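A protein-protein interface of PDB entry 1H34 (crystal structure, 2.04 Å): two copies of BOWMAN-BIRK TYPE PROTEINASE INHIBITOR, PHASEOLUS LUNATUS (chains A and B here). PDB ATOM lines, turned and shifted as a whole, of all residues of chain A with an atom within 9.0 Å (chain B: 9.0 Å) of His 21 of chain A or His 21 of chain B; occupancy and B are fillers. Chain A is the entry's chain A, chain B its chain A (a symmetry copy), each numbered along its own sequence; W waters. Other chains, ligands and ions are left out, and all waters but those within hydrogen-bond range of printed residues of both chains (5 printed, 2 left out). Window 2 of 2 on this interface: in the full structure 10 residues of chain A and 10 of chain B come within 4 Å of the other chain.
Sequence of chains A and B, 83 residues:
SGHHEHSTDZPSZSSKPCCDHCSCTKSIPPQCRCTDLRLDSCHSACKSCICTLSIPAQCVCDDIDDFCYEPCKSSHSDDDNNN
His 21 of chain A touches its own counterpart, His 21 of chain B. Arg 33 of chain A touches Thr 35 of chain B, and with the chains exchanged Thr 35 of chain A touches Arg 33 of chain B. Arg 33 of chain A touches Asp 36 of chain B, and with the chains exchanged Asp 36 of chain A touches Arg 33 of chain B. Thr 35 of chain B touches its own counterpart, Thr 35 of chain A.
Among the printed residues, pairs that only touch across the chains: His 21 of chain A with His 21 of chain B (3.3 Å), Thr 35 of chain A with Thr 35 of chain B (3.3 Å), Arg 33 of chain A with Asp 36 of chain B (3.98 Å) and Asp 36 of chain A with Arg 33 of chain B (3.98 Å).
Water W1 bridges the guanidinium group (NH2) of Arg 33 of chain B (2.6 Å) and the side-chain carboxylate (OD1) of Asp 36 of chain A (3.0 Å). Water W3 bridges a ring nitrogen (NE2) of His 21 of chain B (2.9 Å) and a ring nitrogen (NE2) of His 21 of chain A (2.9 Å). Water W2 bridges N of Leu 37 of chain A (3.1 Å) and NH2 of Arg 33 of chain B (3.5 Å). Water W5 bridges the backbone NH of Leu 37 of chain B and the guanidinium group of Arg 33 of chain A.
SG of Cys 24 of chain B is disulfide-bonded to SG of Cys 32 of chain B, 2.0 Å away. The side-chain sulfur (SG) of Cys 34 of chain A is disulfide-bonded to the side-chain sulfur (SG) of Cys 19 of chain A (2.1 Å). The side-chain sulfur (SG) of Cys 72 of chain B forms a disulfide with the side-chain sulfur (SG) of Cys 18 of chain B, 2.0 Å away.
The guanidinium group (NH1) of Arg 33 of chain A is in hydrogen-bond range of the backbone carbonyl oxygen (O) of Thr 35 of chain B (2.8 Å). O of Thr 35 of chain A lies within hydrogen-bond range of NH1 of Arg 33 of chain B.
Hydrophobic or aromatic side chains of chain A that line the printed part of chain B: His 21. Of the 20 printed residues of chain B, 4 touch a printed residue of chain A. Hydrophobic or aromatic side chains of chain B within 4 Å of the printed part of chain A: His 21. Among the printed residues, 6 pairs touch across the chains. Among the printed residues, no Asp or Glu carboxylate lies within 4 Å of a Lys or Arg side-chain nitrogen of the other chain.
Of chain B, only His 21 (3.3 Å) comes within 4 Å of His 21 of chain A. Cys 22 of chain A touches none of the printed residues of chain B. Of the printed residues of chain B, Arg 33 of chain A touches Thr 35 (2.8 Å) and Asp 36 (3.98 Å). Cys 18 of chain B touches none of the printed residues of chain A. Of chain A, only His 21 comes within 4 Å of His 21 of chain B. Of the printed residues of chain A, Thr 35 of chain B touches Arg 33 (2.8 Å) and Thr 35 (3.3 Å). Of the printed residues of chain A, Asp 36 of chain B touches Arg 33 (3.98 Å). The nearest residue of chain B that does not touch His 21 of chain A is Ser 23 of chain B (4.3 Å). The nearest residue of chain A that does not touch His 21 of chain B is Ser 23 of chain A (4.3 Å).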
ATOM      1  N   CYS A  18      -3.426   6.720 -35.110  1.00  0.00           N
ATOM      2  CA  CYS A  18      -2.296   7.157 -35.911  1.00  0.00           C
ATOM      3  C   CYS A  18      -1.192   7.536 -34.923  1.00  0.00           C
ATOM      4  O   CYS A  18      -1.506   7.669 -33.741  1.00  0.00           O
ATOM      5  CB  CYS A  18      -2.664   8.290 -36.856  1.00  0.00           C
ATOM      6  SG  CYS A  18      -3.141   9.866 -36.103  1.00  0.00           S
ATOM      7  N   CYS A  19       0.035   7.674 -35.415  1.00  0.00           N
ATOM      8  CA  CYS A  19       1.124   7.995 -34.515  1.00  0.00           C
ATOM      9  C   CYS A  19       2.155   8.793 -35.279  1.00  0.00           C
ATOM     10  O   CYS A  19       2.543   8.369 -36.365  1.00  0.00           O
ATOM     11  CB  CYS A  19       1.768   6.711 -33.966  1.00  0.00           C
ATOM     12  SG  CYS A  19       3.173   7.035 -32.883  1.00  0.00           S
ATOM     13  N   ASP A  20       2.613   9.927 -34.762  1.00  0.00           N
ATOM     14  CA  ASP A  20       3.542  10.665 -35.625  1.00  0.00           C
ATOM     15  C   ASP A  20       4.977  10.272 -35.379  1.00  0.00           C
ATOM     16  O   ASP A  20       5.898  10.317 -36.180  1.00  0.00           O
ATOM     17  CB  ASP A  20       3.401  12.178 -35.375  1.00  0.00           C
ATOM     18  CG  ASP A  20       2.253  12.682 -36.242  1.00  0.00           C
ATOM     19  OD1 ASP A  20       2.071  12.088 -37.327  1.00  0.00           O
ATOM     20  OD2 ASP A  20       1.597  13.622 -35.776  1.00  0.00           O
ATOM     21  N   HIS A  21       5.176   9.888 -34.119  1.00  0.00           N
ATOM     22  CA  HIS A  21       6.487   9.415 -33.758  1.00  0.00           C
ATOM     23  C   HIS A  21       6.404   8.071 -33.035  1.00  0.00           C
ATOM     24  O   HIS A  21       5.945   7.999 -31.894  1.00  0.00           O
ATOM     25  CB  HIS A  21       7.156  10.470 -32.878  1.00  0.00           C
ATOM     26  CG  HIS A  21       8.588  10.050 -32.742  1.00  0.00           C
ATOM     27  ND1 HIS A  21       9.220   9.886 -31.535  1.00  0.00           N
ATOM     28  CD2 HIS A  21       9.473   9.738 -33.719  1.00  0.00           C
ATOM     29  CE1 HIS A  21      10.457   9.500 -31.788  1.00  0.00           C
ATOM     30  NE2 HIS A  21      10.647   9.402 -33.090  1.00  0.00           N
ATOM     31  N   CYS A  22       6.861   7.011 -33.684  1.00  0.00           N
ATOM     32  CA  CYS A  22       6.951   5.680 -33.070  1.00  0.00           C
ATOM     33  C   CYS A  22       8.376   5.273 -32.725  1.00  0.00           C
ATOM     34  O   CYS A  22       9.298   5.440 -33.518  1.00  0.00           O
ATOM     35  CB  CYS A  22       6.310   4.696 -34.041  1.00  0.00           C
ATOM     36  SG  CYS A  22       6.121   3.007 -33.412  1.00  0.00           S
ATOM     37  N   SER A  23       8.643   4.741 -31.538  1.00  0.00           N
ATOM     38  CA  SER A  23       9.897   4.185 -31.102  1.00  0.00           C
ATOM     39  C   SER A  23       9.770   2.657 -30.982  1.00  0.00           C
ATOM     40  O   SER A  23       8.845   2.196 -30.303  1.00  0.00           O
ATOM     41  CB  SER A  23      10.333   4.718 -29.740  1.00  0.00           C
ATOM     42  OG  SER A  23      11.521   5.488 -29.791  1.00  0.00           O
ATOM     43  N   CYS A  24      10.664   1.915 -31.607  1.00  0.00           N
ATOM     44  CA  CYS A  24      10.665   0.456 -31.599  1.00  0.00           C
ATOM     45  C   CYS A  24      12.007  -0.119 -31.170  1.00  0.00           C
ATOM     46  O   CYS A  24      13.061   0.407 -31.519  1.00  0.00           O
ATOM     47  CB  CYS A  24      10.370  -0.110 -32.984  1.00  0.00           C
ATOM     48  SG  CYS A  24       8.736   0.122 -33.628  1.00  0.00           S
ATOM     49  N   CYS A  32       7.251  -1.717 -29.790  1.00  0.00           N
ATOM     50  CA  CYS A  32       7.019  -0.376 -30.296  1.00  0.00           C
ATOM     51  C   CYS A  32       6.045   0.408 -29.410  1.00  0.00           C
ATOM     52  O   CYS A  32       5.067  -0.187 -28.948  1.00  0.00           O
ATOM     53  CB  CYS A  32       6.424  -0.465 -31.702  1.00  0.00           C
ATOM     54  SG  CYS A  32       7.492  -1.300 -32.905  1.00  0.00           S
ATOM     55  N   ARG A  33       6.328   1.686 -29.206  1.00  0.00           N
ATOM     56  CA  ARG A  33       5.351   2.598 -28.612  1.00  0.00           C
ATOM     57  C   ARG A  33       5.267   3.936 -29.350  1.00  0.00           C
ATOM     58  O   ARG A  33       6.173   4.373 -30.053  1.00  0.00           O
ATOM     59  CB  ARG A  33       5.656   2.915 -27.151  1.00  0.00           C
ATOM     60  CG  ARG A  33       7.014   3.491 -26.877  1.00  0.00           C
ATOM     61  CD  ARG A  33       7.269   3.751 -25.373  1.00  0.00           C
ATOM     62  NE  ARG A  33       8.610   4.383 -25.367  1.00  0.00           N
ATOM     63  CZ  ARG A  33       8.812   5.669 -25.112  1.00  0.00           C
ATOM     64  NH1 ARG A  33       7.767   6.448 -24.828  1.00  0.00           N
ATOM     65  NH2 ARG A  33      10.043   6.172 -25.135  1.00  0.00           N
ATOM     66  N   CYS A  34       4.136   4.595 -29.149  1.00  0.00           N
ATOM     67  CA  CYS A  34       3.941   5.945 -29.692  1.00  0.00           C
ATOM     68  C   CYS A  34       4.402   6.922 -28.633  1.00  0.00           C
ATOM     69  O   CYS A  34       3.921   6.854 -27.497  1.00  0.00           O
ATOM     70  CB  CYS A  34       2.479   6.196 -30.056  1.00  0.00           C
ATOM     71  SG  CYS A  34       2.195   7.639 -31.119  1.00  0.00           S
ATOM     72  N   THR A  35       5.320   7.838 -28.948  1.00  0.00           N
ATOM     73  CA  THR A  35       5.653   8.813 -27.919  1.00  0.00           C
ATOM     74  C   THR A  35       4.817  10.084 -28.047  1.00  0.00           C
ATOM     75  O   THR A  35       5.060  11.051 -27.304  1.00  0.00           O
ATOM     76  CB  THR A  35       7.140   9.213 -27.998  1.00  0.00           C
ATOM     77  OG1 THR A  35       7.321   9.860 -29.255  1.00  0.00           O
ATOM     78  CG2 THR A  35       8.049   7.994 -27.998  1.00  0.00           C
ATOM     79  N   ASP A  36       3.875  10.134 -28.971  1.00  0.00           N
ATOM     80  CA  ASP A  36       3.130  11.380 -29.195  1.00  0.00           C
ATOM     81  C   ASP A  36       2.465  11.884 -27.916  1.00  0.00           C
ATOM     82  O   ASP A  36       1.952  11.088 -27.132  1.00  0.00           O
ATOM     83  CB  ASP A  36       2.014  11.196 -30.224  1.00  0.00           C
ATOM     84  CG  ASP A  36       2.498  10.829 -31.608  1.00  0.00           C
ATOM     85  OD1 ASP A  36       3.722  10.823 -31.845  1.00  0.00           O
ATOM     86  OD2 ASP A  36       1.634  10.522 -32.446  1.00  0.00           O
ATOM     87  N   LEU A  37       2.453  13.184 -27.718  1.00  0.00           N
ATOM     88  CA  LEU A  37       1.644  13.845 -26.691  1.00  0.00           C
ATOM     89  C   LEU A  37       0.459  14.444 -27.430  1.00  0.00           C
ATOM     90  O   LEU A  37       0.759  15.250 -28.332  1.00  0.00           O
ATOM     91  CB  LEU A  37       2.464  14.934 -26.054  1.00  0.00           C
ATOM     92  CG  LEU A  37       2.897  14.968 -24.622  1.00  0.00           C
ATOM     93  CD1 LEU A  37       3.390  16.368 -24.261  1.00  0.00           C
ATOM     94  CD2 LEU A  37       1.753  14.571 -23.707  1.00  0.00           C
ATOM     95  N   ARG A  38      -0.786  14.117 -27.138  1.00  0.00           N
ATOM     96  CA  ARG A  38      -1.915  14.600 -27.919  1.00  0.00           C
ATOM     97  C   ARG A  38      -2.908  15.415 -27.088  1.00  0.00           C
ATOM     98  O   ARG A  38      -3.015  15.248 -25.882  1.00  0.00           O
ATOM     99  CB  ARG A  38      -2.706  13.457 -28.556  1.00  0.00           C
ATOM    100  CG  ARG A  38      -1.964  12.612 -29.574  1.00  0.00           C
ATOM    101  CD  ARG A  38      -2.669  11.258 -29.721  1.00  0.00           C
ATOM    102  NE  ARG A  38      -3.982  11.463 -30.337  1.00  0.00           N
ATOM    103  CZ  ARG A  38      -4.263  11.147 -31.594  1.00  0.00           C
ATOM    104  NH1 ARG A  38      -3.354  10.605 -32.393  1.00  0.00           N
ATOM    105  NH2 ARG A  38      -5.474  11.371 -32.069  1.00  0.00           N
ATOM    106  N   CYS A  61      -0.220   7.795 -24.924  1.00  0.00           N
ATOM    107  CA  CYS A  61      -0.571   6.365 -24.910  1.00  0.00           C
ATOM    108  C   CYS A  61       0.625   5.555 -24.471  1.00  0.00           C
ATOM    109  O   CYS A  61       1.705   5.642 -25.096  1.00  0.00           O
ATOM    110  CB  CYS A  61      -1.011   5.867 -26.285  1.00  0.00           C
ATOM    111  SG  CYS A  61      -1.746   4.203 -26.319  1.00  0.00           S
ATOM    112  N   CYS A  68       3.914  -0.136 -35.276  1.00  0.00           N
ATOM    113  CA  CYS A  68       3.574   1.272 -35.207  1.00  0.00           C
ATOM    114  C   CYS A  68       2.260   1.632 -35.867  1.00  0.00           C
ATOM    115  O   CYS A  68       1.953   1.139 -36.960  1.00  0.00           O
ATOM    116  CB  CYS A  68       4.666   2.054 -35.937  1.00  0.00           C
ATOM    117  SG  CYS A  68       6.253   1.908 -35.117  1.00  0.00           S
ATOM    118  N   TYR A  69       1.443   2.509 -35.279  1.00  0.00           N
ATOM    119  CA  TYR A  69       0.270   2.977 -36.053  1.00  0.00           C
ATOM    120  C   TYR A  69       0.760   3.836 -37.215  1.00  0.00           C
ATOM    121  O   TYR A  69       1.883   4.368 -37.187  1.00  0.00           O
ATOM    122  CB  TYR A  69      -0.734   3.732 -35.185  1.00  0.00           C
ATOM    123  CG  TYR A  69      -1.361   2.806 -34.154  1.00  0.00           C
ATOM    124  CD1 TYR A  69      -2.512   2.089 -34.431  1.00  0.00           C
ATOM    125  CD2 TYR A  69      -0.777   2.658 -32.901  1.00  0.00           C
ATOM    126  CE1 TYR A  69      -3.076   1.246 -33.485  1.00  0.00           C
ATOM    127  CE2 TYR A  69      -1.339   1.809 -31.958  1.00  0.00           C
ATOM    128  CZ  TYR A  69      -2.483   1.105 -32.247  1.00  0.00           C
ATOM    129  OH  TYR A  69      -3.045   0.266 -31.305  1.00  0.00           O
ATOM    130  N   GLU A  70      -0.024   3.965 -38.274  1.00  0.00           N
ATOM    131  CA  GLU A  70       0.381   4.809 -39.401  1.00  0.00           C
ATOM    132  C   GLU A  70       0.451   6.279 -39.019  1.00  0.00           C
ATOM    133  O   GLU A  70      -0.170   6.722 -38.059  1.00  0.00           O
ATOM    134  CB  GLU A  70      -0.622   4.660 -40.555  1.00  0.00           C
ATOM    135  CG  GLU A  70      -2.036   4.554 -39.996  1.00  0.00           C
ATOM    136  CD  GLU A  70      -3.094   5.030 -40.966  1.00  0.00           C
ATOM    137  OE1 GLU A  70      -2.968   6.172 -41.460  1.00  0.00           O
ATOM    138  OE2 GLU A  70      -4.044   4.260 -41.218  1.00  0.00           O
ATOM    139  N   PRO A  71       1.232   7.038 -39.769  1.00  0.00           N
ATOM    140  CA  PRO A  71       1.420   8.461 -39.466  1.00  0.00           C
ATOM    141  C   PRO A  71       0.085   9.193 -39.378  1.00  0.00           C
ATOM    142  O   PRO A  71      -0.916   8.734 -39.922  1.00  0.00           O
ATOM    143  CB  PRO A  71       2.255   8.956 -40.650  1.00  0.00           C
ATOM    144  CG  PRO A  71       3.018   7.732 -41.065  1.00  0.00           C
ATOM    145  CD  PRO A  71       2.004   6.615 -40.952  1.00  0.00           C
ATOM    146  N   CYS A  72       0.091  10.313 -38.666  1.00  0.00           N
ATOM    147  CA  CYS A  72      -1.094  11.145 -38.515  1.00  0.00           C
ATOM    148  C   CYS A  72      -1.176  12.166 -39.648  1.00  0.00           C
ATOM    149  O   CYS A  72      -0.662  11.917 -40.742  1.00  0.00           O
ATOM    150  CB  CYS A  72      -1.084  11.862 -37.169  1.00  0.00           C
ATOM    151  SG  CYS A  72      -1.374  10.798 -35.746  1.00  0.00           S
ATOM    152  N   CYS B  18      17.805  12.991 -16.317  1.00  0.00           N
ATOM    153  CA  CYS B  18      18.458  12.439 -17.491  1.00  0.00           C
ATOM    154  C   CYS B  18      17.340  12.062 -18.464  1.00  0.00           C
ATOM    155  O   CYS B  18      16.192  12.022 -18.025  1.00  0.00           O
ATOM    156  CB  CYS B  18      19.369  11.272 -17.149  1.00  0.00           C
ATOM    157  SG  CYS B  18      18.581   9.776 -16.498  1.00  0.00           S
ATOM    158  N   CYS B  19      17.693  11.823 -19.723  1.00  0.00           N
ATOM    159  CA  CYS B  19      16.667  11.497 -20.693  1.00  0.00           C
ATOM    160  C   CYS B  19      17.273  10.594 -21.743  1.00  0.00           C
ATOM    161  O   CYS B  19      18.335  10.925 -22.264  1.00  0.00           O
ATOM    162  CB  CYS B  19      16.129  12.774 -21.360  1.00  0.00           C
ATOM    163  SG  CYS B  19      14.888  12.440 -22.625  1.00  0.00           S
ATOM    164  N   ASP B  20      16.647   9.471 -22.073  1.00  0.00           N
ATOM    165  CA  ASP B  20      17.364   8.628 -23.035  1.00  0.00           C
ATOM    166  C   ASP B  20      16.993   8.952 -24.461  1.00  0.00           C
ATOM    167  O   ASP B  20      17.690   8.804 -25.453  1.00  0.00           O
ATOM    168  CB  ASP B  20      17.043   7.144 -22.774  1.00  0.00           C
ATOM    169  CG  ASP B  20      17.995   6.653 -21.690  1.00  0.00           C
ATOM    170  OD1 ASP B  20      19.126   7.186 -21.655  1.00  0.00           O
ATOM    171  OD2 ASP B  20      17.546   5.784 -20.931  1.00  0.00           O
ATOM    172  N   HIS B  21      15.744   9.404 -24.556  1.00  0.00           N
ATOM    173  CA  HIS B  21      15.276   9.822 -25.851  1.00  0.00           C
ATOM    174  C   HIS B  21      14.643  11.213 -25.783  1.00  0.00           C
ATOM    175  O   HIS B  21      13.564  11.383 -25.217  1.00  0.00           O
ATOM    176  CB  HIS B  21      14.272   8.789 -26.360  1.00  0.00           C
ATOM    177  CG  HIS B  21      14.011   9.134 -27.795  1.00  0.00           C
ATOM    178  ND1 HIS B  21      12.757   9.338 -28.312  1.00  0.00           N
ATOM    179  CD2 HIS B  21      14.907   9.332 -28.793  1.00  0.00           C
ATOM    180  CE1 HIS B  21      12.902   9.635 -29.590  1.00  0.00           C
ATOM    181  NE2 HIS B  21      14.180   9.639 -29.916  1.00  0.00           N
ATOM    182  N   CYS B  22      15.302  12.201 -26.369  1.00  0.00           N
ATOM    183  CA  CYS B  22      14.759  13.561 -26.482  1.00  0.00           C
ATOM    184  C   CYS B  22      14.291  13.907 -27.888  1.00  0.00           C
ATOM    185  O   CYS B  22      14.974  13.636 -28.871  1.00  0.00           O
ATOM    186  CB  CYS B  22      15.846  14.517 -26.005  1.00  0.00           C
ATOM    187  SG  CYS B  22      15.338  16.250 -25.862  1.00  0.00           S
ATOM    188  N   SER B  23      13.115  14.497 -28.067  1.00  0.00           N
ATOM    189  CA  SER B  23      12.585  15.005 -29.304  1.00  0.00           C
ATOM    190  C   SER B  23      12.566  16.544 -29.263  1.00  0.00           C
ATOM    191  O   SER B  23      12.015  17.099 -28.306  1.00  0.00           O
ATOM    192  CB  SER B  23      11.156  14.537 -29.567  1.00  0.00           C
ATOM    193  OG  SER B  23      11.038  13.698 -30.702  1.00  0.00           O
ATOM    194  N   CYS B  24      13.136  17.192 -30.261  1.00  0.00           N
ATOM    195  CA  CYS B  24      13.212  18.646 -30.355  1.00  0.00           C
ATOM    196  C   CYS B  24      12.679  19.168 -31.680  1.00  0.00           C
ATOM    197  O   CYS B  24      12.886  18.562 -32.728  1.00  0.00           O
ATOM    198  CB  CYS B  24      14.651  19.138 -30.236  1.00  0.00           C
ATOM    199  SG  CYS B  24      15.447  18.960 -28.664  1.00  0.00           S
ATOM    200  N   CYS B  32      11.896  21.122 -26.921  1.00  0.00           N
ATOM    201  CA  CYS B  32      12.346  19.767 -26.657  1.00  0.00           C
ATOM    202  C   CYS B  32      11.522  19.099 -25.550  1.00  0.00           C
ATOM    203  O   CYS B  32      11.200  19.777 -24.570  1.00  0.00           O
ATOM    204  CB  CYS B  32      13.808  19.801 -26.213  1.00  0.00           C
ATOM    205  SG  CYS B  32      14.940  20.494 -27.447  1.00  0.00           S
ATOM    206  N   ARG B  33      11.218  17.821 -25.728  1.00  0.00           N
ATOM    207  CA  ARG B  33      10.677  17.007 -24.640  1.00  0.00           C
ATOM    208  C   ARG B  33      11.341  15.632 -24.547  1.00  0.00           C
ATOM    209  O   ARG B  33      11.920  15.099 -25.488  1.00  0.00           O
ATOM    210  CB  ARG B  33       9.175  16.767 -24.777  1.00  0.00           C
ATOM    211  CG  ARG B  33       8.729  16.133 -26.061  1.00  0.00           C
ATOM    212  CD  ARG B  33       7.194  15.955 -26.147  1.00  0.00           C
ATOM    213  NE  ARG B  33       7.013  15.249 -27.437  1.00  0.00           N
ATOM    214  CZ  ARG B  33       6.665  13.971 -27.530  1.00  0.00           C
ATOM    215  NH1 ARG B  33       6.446  13.274 -26.414  1.00  0.00           N
ATOM    216  NH2 ARG B  33       6.530  13.399 -28.723  1.00  0.00           N
ATOM    217  N   CYS B  34      11.221  15.053 -23.362  1.00  0.00           N
ATOM    218  CA  CYS B  34      11.703  13.684 -23.136  1.00  0.00           C
ATOM    219  C   CYS B  34      10.547  12.752 -23.426  1.00  0.00           C
ATOM    220  O   CYS B  34       9.474  12.920 -22.839  1.00  0.00           O
ATOM    221  CB  CYS B  34      12.203  13.496 -21.705  1.00  0.00           C
ATOM    222  SG  CYS B  34      13.205  12.006 -21.438  1.00  0.00           S
ATOM    223  N   THR B  35      10.712  11.767 -24.311  1.00  0.00           N
ATOM    224  CA  THR B  35       9.599  10.843 -24.475  1.00  0.00           C
ATOM    225  C   THR B  35       9.741   9.616 -23.577  1.00  0.00           C
ATOM    226  O   THR B  35       8.922   8.685 -23.682  1.00  0.00           O
ATOM    227  CB  THR B  35       9.500  10.353 -25.934  1.00  0.00           C
ATOM    228  OG1 THR B  35      10.692   9.618 -26.199  1.00  0.00           O
ATOM    229  CG2 THR B  35       9.476  11.515 -26.914  1.00  0.00           C
ATOM    230  N   ASP B  36      10.754   9.560 -22.731  1.00  0.00           N
ATOM    231  CA  ASP B  36      10.981   8.348 -21.935  1.00  0.00           C
ATOM    232  C   ASP B  36       9.752   7.966 -21.115  1.00  0.00           C
ATOM    233  O   ASP B  36       9.073   8.838 -20.577  1.00  0.00           O
ATOM    234  CB  ASP B  36      12.131   8.530 -20.942  1.00  0.00           C
ATOM    235  CG  ASP B  36      13.475   8.780 -21.585  1.00  0.00           C
ATOM    236  OD1 ASP B  36      13.584   8.699 -22.824  1.00  0.00           O
ATOM    237  OD2 ASP B  36      14.414   9.082 -20.831  1.00  0.00           O
ATOM    238  N   LEU B  37       9.482   6.685 -21.000  1.00  0.00           N
ATOM    239  CA  LEU B  37       8.508   6.138 -20.051  1.00  0.00           C
ATOM    240  C   LEU B  37       9.332   5.561 -18.910  1.00  0.00           C
ATOM    241  O   LEU B  37      10.150   4.683 -19.247  1.00  0.00           O
ATOM    242  CB  LEU B  37       7.728   5.046 -20.732  1.00  0.00           C
ATOM    243  CG  LEU B  37       6.259   5.078 -21.016  1.00  0.00           C
ATOM    244  CD1 LEU B  37       5.770   3.678 -21.379  1.00  0.00           C
ATOM    245  CD2 LEU B  37       5.493   5.598 -19.813  1.00  0.00           C
ATOM    246  N   ARG B  38       9.190   5.978 -17.666  1.00  0.00           N
ATOM    247  CA  ARG B  38      10.055   5.511 -16.593  1.00  0.00           C
ATOM    248  C   ARG B  38       9.286   4.809 -15.472  1.00  0.00           C
ATOM    249  O   ARG B  38       8.110   5.059 -15.255  1.00  0.00           O
ATOM    250  CB  ARG B  38      10.835   6.656 -15.944  1.00  0.00           C
ATOM    251  CG  ARG B  38      11.818   7.390 -16.837  1.00  0.00           C
ATOM    252  CD  ARG B  38      12.115   8.770 -16.237  1.00  0.00           C
ATOM    253  NE  ARG B  38      12.852   8.601 -14.983  1.00  0.00           N
ATOM    254  CZ  ARG B  38      14.147   8.852 -14.850  1.00  0.00           C
ATOM    255  NH1 ARG B  38      14.877   9.289 -15.867  1.00  0.00           N
ATOM    256  NH2 ARG B  38      14.732   8.668 -13.681  1.00  0.00           N
ATOM    257  N   CYS B  61       7.296  12.385 -18.408  1.00  0.00           N
ATOM    258  CA  CYS B  61       7.401  13.831 -18.149  1.00  0.00           C
ATOM    259  C   CYS B  61       6.887  14.597 -19.345  1.00  0.00           C
ATOM    260  O   CYS B  61       7.390  14.408 -20.474  1.00  0.00           O
ATOM    261  CB  CYS B  61       8.840  14.264 -17.883  1.00  0.00           C
ATOM    262  SG  CYS B  61       9.046  15.962 -17.262  1.00  0.00           S
ATOM    263  N   CYS B  68      17.600  19.389 -24.058  1.00  0.00           N
ATOM    264  CA  CYS B  68      17.486  18.011 -23.624  1.00  0.00           C
ATOM    265  C   CYS B  68      18.258  17.685 -22.362  1.00  0.00           C
ATOM    266  O   CYS B  68      19.403  18.125 -22.199  1.00  0.00           O
ATOM    267  CB  CYS B  68      18.052  17.122 -24.732  1.00  0.00           C
ATOM    268  SG  CYS B  68      17.081  17.228 -26.234  1.00  0.00           S
ATOM    269  N   TYR B  69      17.708  16.896 -21.436  1.00  0.00           N
ATOM    270  CA  TYR B  69      18.572  16.448 -20.319  1.00  0.00           C
ATOM    271  C   TYR B  69      19.626  15.490 -20.868  1.00  0.00           C
ATOM    272  O   TYR B  69      19.451  14.896 -21.946  1.00  0.00           O
ATOM    273  CB  TYR B  69      17.771  15.809 -19.188  1.00  0.00           C
ATOM    274  CG  TYR B  69      16.866  16.833 -18.520  1.00  0.00           C
ATOM    275  CD1 TYR B  69      17.302  17.596 -17.451  1.00  0.00           C
ATOM    276  CD2 TYR B  69      15.570  17.027 -18.984  1.00  0.00           C
ATOM    277  CE1 TYR B  69      16.470  18.528 -16.849  1.00  0.00           C
ATOM    278  CE2 TYR B  69      14.742  17.964 -18.385  1.00  0.00           C
ATOM    279  CZ  TYR B  69      15.187  18.714 -17.323  1.00  0.00           C
ATOM    280  OH  TYR B  69      14.359  19.641 -16.724  1.00  0.00           O
ATOM    281  N   GLU B  70      20.751  15.339 -20.188  1.00  0.00           N
ATOM    282  CA  GLU B  70      21.780  14.403 -20.649  1.00  0.00           C
ATOM    283  C   GLU B  70      21.308  12.959 -20.587  1.00  0.00           C
ATOM    284  O   GLU B  70      20.395  12.613 -19.845  1.00  0.00           O
ATOM    285  CB  GLU B  70      23.038  14.535 -19.778  1.00  0.00           C
ATOM    286  CG  GLU B  70      22.637  14.758 -18.325  1.00  0.00           C
ATOM    287  CD  GLU B  70      23.683  14.283 -17.342  1.00  0.00           C
ATOM    288  OE1 GLU B  70      24.095  13.105 -17.444  1.00  0.00           O
ATOM    289  OE2 GLU B  70      24.076  15.088 -16.473  1.00  0.00           O
ATOM    290  N   PRO B  71      21.928  12.110 -21.389  1.00  0.00           N
ATOM    291  CA  PRO B  71      21.526  10.700 -21.455  1.00  0.00           C
ATOM    292  C   PRO B  71      21.536  10.053 -20.074  1.00  0.00           C
ATOM    293  O   PRO B  71      22.206  10.533 -19.164  1.00  0.00           O
ATOM    294  CB  PRO B  71      22.586  10.083 -22.371  1.00  0.00           C
ATOM    295  CG  PRO B  71      22.990  11.232 -23.248  1.00  0.00           C
ATOM    296  CD  PRO B  71      23.046  12.411 -22.302  1.00  0.00           C
ATOM    297  N   CYS B  72      20.764   8.983 -19.937  1.00  0.00           N
ATOM    298  CA  CYS B  72      20.689   8.231 -18.693  1.00  0.00           C
ATOM    299  C   CYS B  72      21.764   7.147 -18.659  1.00  0.00           C
ATOM    300  O   CYS B  72      22.810   7.295 -19.295  1.00  0.00           O
ATOM    301  CB  CYS B  72      19.310   7.602 -18.521  1.00  0.00           C
ATOM    302  SG  CYS B  72      17.988   8.770 -18.158  1.00  0.00           S
HETATM  303  O   HOH W   1       5.793  12.833 -31.175  1.00  0.00           O
HETATM  304  O   HOH W   2       3.716  15.092 -29.869  1.00  0.00           O
HETATM  305  O   HOH W   3      13.506   9.450 -32.714  1.00  0.00           O
HETATM  306  O   HOH W   4      12.587   6.622 -24.686  1.00  0.00           O
HETATM  307  O   HOH W   5      11.376   4.574 -22.348  1.00  0.00           O
